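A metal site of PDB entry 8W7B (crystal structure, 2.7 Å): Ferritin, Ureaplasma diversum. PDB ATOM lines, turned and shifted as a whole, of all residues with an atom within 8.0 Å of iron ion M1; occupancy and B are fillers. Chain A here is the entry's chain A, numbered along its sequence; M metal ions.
Merely in contact with iron ion M1: Lys 141 (3.9 Å).
The nearest printed residue that does not touch iron ion M1 is Trp 134 (4.6 Å).
OD2 of Asp 138 binds iron ion M1 (1.9 Å).
OD2 of Asp 60 binds iron ion M1 (2.1 Å).
OD2 of Asp 142 is bound to iron ion M1.
Iron ion M1 is bound by NE2 of His 65.
The side-chain carboxylate of Asp 138 lies within salt-bridge range of the side-chain amino group of Lys 141 (3.5 Å).
OD1 of Asp 138 is in salt-bridge range of NH2 of Arg 137 (3.2 Å).
The side-chain carboxylate (OD1) of Asp 142 lies within salt-bridge range of the side-chain amino group (NZ) of Lys 141 (3.0 Å).
The side-chain amino group of Lys 61 sits close to the side-chain carboxylate of Asp 142 (3.6 Å).
The side-chain amide oxygen (OD1) of Asn 27 lies close to a ring nitrogen (ND1) of His 65, 3.2 Å away.
The backbone carbonyl oxygen (O) of His 65 sits at hydrogen-bond distance from the side-chain hydroxyl (OH) of Tyr 135.
The side-chain amino group of Lys 141 lies within salt-bridge range of the side-chain carboxylate of Glu 145 (3.6 Å).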
ATOM      1  N   ASN A  27      16.625 -27.109 -23.674  1.00  0.00           N
ATOM      2  CA  ASN A  27      15.557 -26.336 -23.047  1.00  0.00           C
ATOM      3  C   ASN A  27      14.945 -27.059 -21.856  1.00  0.00           C
ATOM      4  O   ASN A  27      14.611 -26.428 -20.843  1.00  0.00           O
ATOM      5  CB  ASN A  27      14.504 -25.991 -24.083  1.00  0.00           C
ATOM      6  CG  ASN A  27      14.937 -24.817 -24.924  1.00  0.00           C
ATOM      7  OD1 ASN A  27      14.721 -23.665 -24.549  1.00  0.00           O
ATOM      8  ND2 ASN A  27      15.619 -25.101 -26.032  1.00  0.00           N
ATOM      9  N   HIS A  56       9.960 -17.729 -14.162  1.00  0.00           N
ATOM     10  CA  HIS A  56       9.295 -17.433 -15.433  1.00  0.00           C
ATOM     11  C   HIS A  56      10.165 -17.860 -16.593  1.00  0.00           C
ATOM     12  O   HIS A  56       9.648 -18.321 -17.627  1.00  0.00           O
ATOM     13  CB  HIS A  56       8.964 -15.942 -15.528  1.00  0.00           C
ATOM     14  CG  HIS A  56       7.813 -15.519 -14.662  1.00  0.00           C
ATOM     15  ND1 HIS A  56       6.803 -16.379 -14.295  1.00  0.00           N
ATOM     16  CD2 HIS A  56       7.524 -14.330 -14.083  1.00  0.00           C
ATOM     17  CE1 HIS A  56       5.933 -15.736 -13.530  1.00  0.00           C
ATOM     18  NE2 HIS A  56       6.344 -14.498 -13.382  1.00  0.00           N
ATOM     19  N   LEU A  57      11.485 -17.711 -16.458  1.00  0.00           N
ATOM     20  CA  LEU A  57      12.403 -18.224 -17.462  1.00  0.00           C
ATOM     21  C   LEU A  57      12.323 -19.734 -17.522  1.00  0.00           C
ATOM     22  O   LEU A  57      12.346 -20.334 -18.598  1.00  0.00           O
ATOM     23  CB  LEU A  57      13.831 -17.788 -17.138  1.00  0.00           C
ATOM     24  CG  LEU A  57      14.622 -16.900 -18.092  1.00  0.00           C
ATOM     25  CD1 LEU A  57      16.003 -16.712 -17.495  1.00  0.00           C
ATOM     26  CD2 LEU A  57      14.736 -17.500 -19.475  1.00  0.00           C
ATOM     27  N   GLU A  59       9.760 -21.729 -16.721  1.00  0.00           N
ATOM     28  CA  GLU A  59       8.523 -22.188 -17.358  1.00  0.00           C
ATOM     29  C   GLU A  59       8.491 -21.862 -18.841  1.00  0.00           C
ATOM     30  O   GLU A  59       7.852 -22.577 -19.624  1.00  0.00           O
ATOM     31  CB  GLU A  59       7.315 -21.591 -16.661  1.00  0.00           C
ATOM     32  CG  GLU A  59       7.056 -22.200 -15.311  1.00  0.00           C
ATOM     33  CD  GLU A  59       6.278 -21.270 -14.430  1.00  0.00           C
ATOM     34  OE1 GLU A  59       5.797 -20.222 -14.942  1.00  0.00           O
ATOM     35  OE2 GLU A  59       6.143 -21.595 -13.228  1.00  0.00           O
ATOM     36  N   ASP A  60       9.162 -20.793 -19.243  1.00  0.00           N
ATOM     37  CA  ASP A  60       9.348 -20.487 -20.650  1.00  0.00           C
ATOM     38  C   ASP A  60      10.137 -21.591 -21.356  1.00  0.00           C
ATOM     39  O   ASP A  60       9.731 -22.087 -22.419  1.00  0.00           O
ATOM     40  CB  ASP A  60      10.039 -19.129 -20.782  1.00  0.00           C
ATOM     41  CG  ASP A  60      10.083 -18.630 -22.201  1.00  0.00           C
ATOM     42  OD1 ASP A  60       9.042 -18.725 -22.904  1.00  0.00           O
ATOM     43  OD2 ASP A  60      11.163 -18.153 -22.600  1.00  0.00           O
ATOM     44  N   LYS A  61      11.266 -22.018 -20.770  1.00  0.00           N
ATOM     45  CA  LYS A  61      12.099 -23.043 -21.405  1.00  0.00           C
ATOM     46  C   LYS A  61      11.392 -24.397 -21.450  1.00  0.00           C
ATOM     47  O   LYS A  61      11.438 -25.099 -22.466  1.00  0.00           O
ATOM     48  CB  LYS A  61      13.439 -23.194 -20.673  1.00  0.00           C
ATOM     49  CG  LYS A  61      14.289 -21.929 -20.574  1.00  0.00           C
ATOM     50  CD  LYS A  61      14.684 -21.412 -21.930  1.00  0.00           C
ATOM     51  CE  LYS A  61      15.327 -20.042 -21.835  1.00  0.00           C
ATOM     52  NZ  LYS A  61      16.150 -19.730 -23.028  1.00  0.00           N
ATOM     53  N   VAL A  64       6.940 -23.430 -24.122  1.00  0.00           N
ATOM     54  CA  VAL A  64       6.864 -23.265 -25.561  1.00  0.00           C
ATOM     55  C   VAL A  64       8.198 -23.521 -26.256  1.00  0.00           C
ATOM     56  O   VAL A  64       8.212 -23.886 -27.437  1.00  0.00           O
ATOM     57  CB  VAL A  64       6.328 -21.861 -25.918  1.00  0.00           C
ATOM     58  CG1 VAL A  64       4.865 -21.765 -25.611  1.00  0.00           C
ATOM     59  CG2 VAL A  64       7.090 -20.792 -25.177  1.00  0.00           C
ATOM     60  N   HIS A  65       9.321 -23.350 -25.549  1.00  0.00           N
ATOM     61  CA  HIS A  65      10.600 -23.658 -26.183  1.00  0.00           C
ATOM     62  C   HIS A  65      10.695 -25.134 -26.574  1.00  0.00           C
ATOM     63  O   HIS A  65      11.202 -25.472 -27.644  1.00  0.00           O
ATOM     64  CB  HIS A  65      11.760 -23.261 -25.269  1.00  0.00           C
ATOM     65  CG  HIS A  65      12.057 -21.781 -25.264  1.00  0.00           C
ATOM     66  ND1 HIS A  65      13.173 -21.242 -25.865  1.00  0.00           N
ATOM     67  CD2 HIS A  65      11.411 -20.748 -24.691  1.00  0.00           C
ATOM     68  CE1 HIS A  65      13.180 -19.934 -25.685  1.00  0.00           C
ATOM     69  NE2 HIS A  65      12.125 -19.605 -24.967  1.00  0.00           N
ATOM     70  N   GLU A 106      22.333 -18.257 -21.221  1.00  0.00           N
ATOM     71  CA  GLU A 106      21.511 -17.727 -22.312  1.00  0.00           C
ATOM     72  C   GLU A 106      22.361 -17.294 -23.503  1.00  0.00           C
ATOM     73  O   GLU A 106      21.894 -17.357 -24.646  1.00  0.00           O
ATOM     74  CB  GLU A 106      20.647 -16.562 -21.828  1.00  0.00           C
ATOM     75  CG  GLU A 106      19.621 -17.010 -20.813  1.00  0.00           C
ATOM     76  CD  GLU A 106      18.480 -17.776 -21.443  1.00  0.00           C
ATOM     77  OE1 GLU A 106      18.000 -17.363 -22.517  1.00  0.00           O
ATOM     78  OE2 GLU A 106      18.086 -18.811 -20.875  1.00  0.00           O
ATOM     79  N   VAL A 109      22.760 -20.239 -25.617  1.00  0.00           N
ATOM     80  CA  VAL A 109      21.545 -20.450 -26.410  1.00  0.00           C
ATOM     81  C   VAL A 109      21.677 -19.774 -27.771  1.00  0.00           C
ATOM     82  O   VAL A 109      21.422 -20.387 -28.823  1.00  0.00           O
ATOM     83  CB  VAL A 109      20.303 -19.966 -25.646  1.00  0.00           C
ATOM     84  CG1 VAL A 109      19.105 -19.814 -26.597  1.00  0.00           C
ATOM     85  CG2 VAL A 109      19.972 -20.908 -24.490  1.00  0.00           C
ATOM     86  N   TRP A 134      11.990 -17.727 -35.020  1.00  0.00           N
ATOM     87  CA  TRP A 134      11.452 -17.497 -33.673  1.00  0.00           C
ATOM     88  C   TRP A 134      12.552 -17.606 -32.616  1.00  0.00           C
ATOM     89  O   TRP A 134      12.694 -16.722 -31.764  1.00  0.00           O
ATOM     90  CB  TRP A 134      10.340 -18.506 -33.360  1.00  0.00           C
ATOM     91  CG  TRP A 134       9.584 -18.190 -32.097  1.00  0.00           C
ATOM     92  CD1 TRP A 134       8.471 -17.418 -32.003  1.00  0.00           C
ATOM     93  CD2 TRP A 134       9.904 -18.611 -30.757  1.00  0.00           C
ATOM     94  NE1 TRP A 134       8.061 -17.347 -30.692  1.00  0.00           N
ATOM     95  CE2 TRP A 134       8.918 -18.056 -29.911  1.00  0.00           C
ATOM     96  CE3 TRP A 134      10.925 -19.391 -30.193  1.00  0.00           C
ATOM     97  CZ2 TRP A 134       8.917 -18.262 -28.519  1.00  0.00           C
ATOM     98  CZ3 TRP A 134      10.918 -19.594 -28.813  1.00  0.00           C
ATOM     99  CH2 TRP A 134       9.921 -19.033 -27.992  1.00  0.00           C
ATOM    100  N   TYR A 135      13.312 -18.688 -32.662  1.00  0.00           N
ATOM    101  CA  TYR A 135      14.374 -18.904 -31.686  1.00  0.00           C
ATOM    102  C   TYR A 135      15.519 -17.912 -31.867  1.00  0.00           C
ATOM    103  O   TYR A 135      16.150 -17.515 -30.871  1.00  0.00           O
ATOM    104  CB  TYR A 135      14.885 -20.345 -31.776  1.00  0.00           C
ATOM    105  CG  TYR A 135      13.852 -21.375 -31.360  1.00  0.00           C
ATOM    106  CD1 TYR A 135      12.881 -21.821 -32.256  1.00  0.00           C
ATOM    107  CD2 TYR A 135      13.851 -21.898 -30.071  1.00  0.00           C
ATOM    108  CE1 TYR A 135      11.932 -22.751 -31.871  1.00  0.00           C
ATOM    109  CE2 TYR A 135      12.928 -22.840 -29.670  1.00  0.00           C
ATOM    110  CZ  TYR A 135      11.961 -23.270 -30.580  1.00  0.00           C
ATOM    111  OH  TYR A 135      11.026 -24.215 -30.174  1.00  0.00           O
ATOM    112  N   ARG A 137      15.118 -14.796 -32.749  1.00  0.00           N
ATOM    113  CA  ARG A 137      14.627 -13.611 -32.068  1.00  0.00           C
ATOM    114  C   ARG A 137      14.583 -13.818 -30.567  1.00  0.00           C
ATOM    115  O   ARG A 137      15.074 -12.973 -29.801  1.00  0.00           O
ATOM    116  CB  ARG A 137      13.245 -13.230 -32.610  1.00  0.00           C
ATOM    117  CG  ARG A 137      12.584 -12.070 -31.879  1.00  0.00           C
ATOM    118  CD  ARG A 137      11.065 -12.154 -31.927  1.00  0.00           C
ATOM    119  NE  ARG A 137      10.574 -13.475 -31.544  1.00  0.00           N
ATOM    120  CZ  ARG A 137      10.508 -13.912 -30.291  1.00  0.00           C
ATOM    121  NH1 ARG A 137      10.047 -15.128 -30.049  1.00  0.00           N
ATOM    122  NH2 ARG A 137      10.899 -13.140 -29.296  1.00  0.00           N
ATOM    123  N   ASP A 138      13.985 -14.917 -30.102  1.00  0.00           N
ATOM    124  CA  ASP A 138      13.855 -15.098 -28.658  1.00  0.00           C
ATOM    125  C   ASP A 138      15.206 -15.229 -27.983  1.00  0.00           C
ATOM    126  O   ASP A 138      15.317 -14.935 -26.783  1.00  0.00           O
ATOM    127  CB  ASP A 138      12.994 -16.314 -28.331  1.00  0.00           C
ATOM    128  CG  ASP A 138      12.221 -16.138 -27.039  1.00  0.00           C
ATOM    129  OD1 ASP A 138      11.413 -15.198 -26.943  1.00  0.00           O
ATOM    130  OD2 ASP A 138      12.440 -16.952 -26.112  1.00  0.00           O
ATOM    131  N   GLY A 139      16.234 -15.660 -28.729  1.00  0.00           N
ATOM    132  CA  GLY A 139      17.576 -15.777 -28.166  1.00  0.00           C
ATOM    133  C   GLY A 139      18.091 -14.465 -27.640  1.00  0.00           C
ATOM    134  O   GLY A 139      18.718 -14.411 -26.576  1.00  0.00           O
ATOM    135  N   LYS A 141      16.003 -11.696 -27.026  1.00  0.00           N
ATOM    136  CA  LYS A 141      15.053 -11.145 -26.053  1.00  0.00           C
ATOM    137  C   LYS A 141      15.288 -11.730 -24.651  1.00  0.00           C
ATOM    138  O   LYS A 141      15.337 -10.983 -23.661  1.00  0.00           O
ATOM    139  CB  LYS A 141      13.617 -11.411 -26.508  1.00  0.00           C
ATOM    140  CG  LYS A 141      12.576 -10.625 -25.682  1.00  0.00           C
ATOM    141  CD  LYS A 141      11.348 -11.462 -25.335  1.00  0.00           C
ATOM    142  CE  LYS A 141      11.730 -12.881 -24.916  1.00  0.00           C
ATOM    143  NZ  LYS A 141      10.745 -13.550 -23.985  1.00  0.00           N
ATOM    144  N   ASP A 142      15.405 -13.047 -24.547  1.00  0.00           N
ATOM    145  CA  ASP A 142      15.629 -13.618 -23.224  1.00  0.00           C
ATOM    146  C   ASP A 142      16.954 -13.144 -22.649  1.00  0.00           C
ATOM    147  O   ASP A 142      17.075 -12.948 -21.438  1.00  0.00           O
ATOM    148  CB  ASP A 142      15.570 -15.145 -23.282  1.00  0.00           C
ATOM    149  CG  ASP A 142      14.133 -15.692 -23.276  1.00  0.00           C
ATOM    150  OD1 ASP A 142      13.194 -14.900 -23.027  1.00  0.00           O
ATOM    151  OD2 ASP A 142      13.936 -16.912 -23.529  1.00  0.00           O
ATOM    152  N   LEU A 143      17.949 -12.934 -23.508  1.00  0.00           N
ATOM    153  CA  LEU A 143      19.238 -12.444 -23.033  1.00  0.00           C
ATOM    154  C   LEU A 143      19.128 -11.002 -22.548  1.00  0.00           C
ATOM    155  O   LEU A 143      19.737 -10.631 -21.548  1.00  0.00           O
ATOM    156  CB  LEU A 143      20.287 -12.573 -24.131  1.00  0.00           C
ATOM    157  CG  LEU A 143      21.702 -12.178 -23.691  1.00  0.00           C
ATOM    158  CD1 LEU A 143      22.497 -13.385 -23.246  1.00  0.00           C
ATOM    159  CD2 LEU A 143      22.420 -11.433 -24.798  1.00  0.00           C
ATOM    160  N   GLU A 145      16.393  -9.512 -21.274  1.00  0.00           N
ATOM    161  CA  GLU A 145      15.694  -9.557 -19.984  1.00  0.00           C
ATOM    162  C   GLU A 145      16.638  -9.972 -18.858  1.00  0.00           C
ATOM    163  O   GLU A 145      16.707  -9.275 -17.834  1.00  0.00           O
ATOM    164  CB  GLU A 145      14.495 -10.510 -20.048  1.00  0.00           C
ATOM    165  CG  GLU A 145      13.386 -10.118 -21.029  1.00  0.00           C
ATOM    166  CD  GLU A 145      12.227 -11.144 -21.107  1.00  0.00           C
ATOM    167  OE1 GLU A 145      12.346 -12.260 -20.545  1.00  0.00           O
ATOM    168  OE2 GLU A 145      11.201 -10.818 -21.751  1.00  0.00           O
HETATM  169 FE    FE M   1      12.008 -17.271 -24.279  1.00  0.00          FE
HETATM  170 FE    FE M   2      16.262 -17.635 -25.685  1.00  0.00          FE
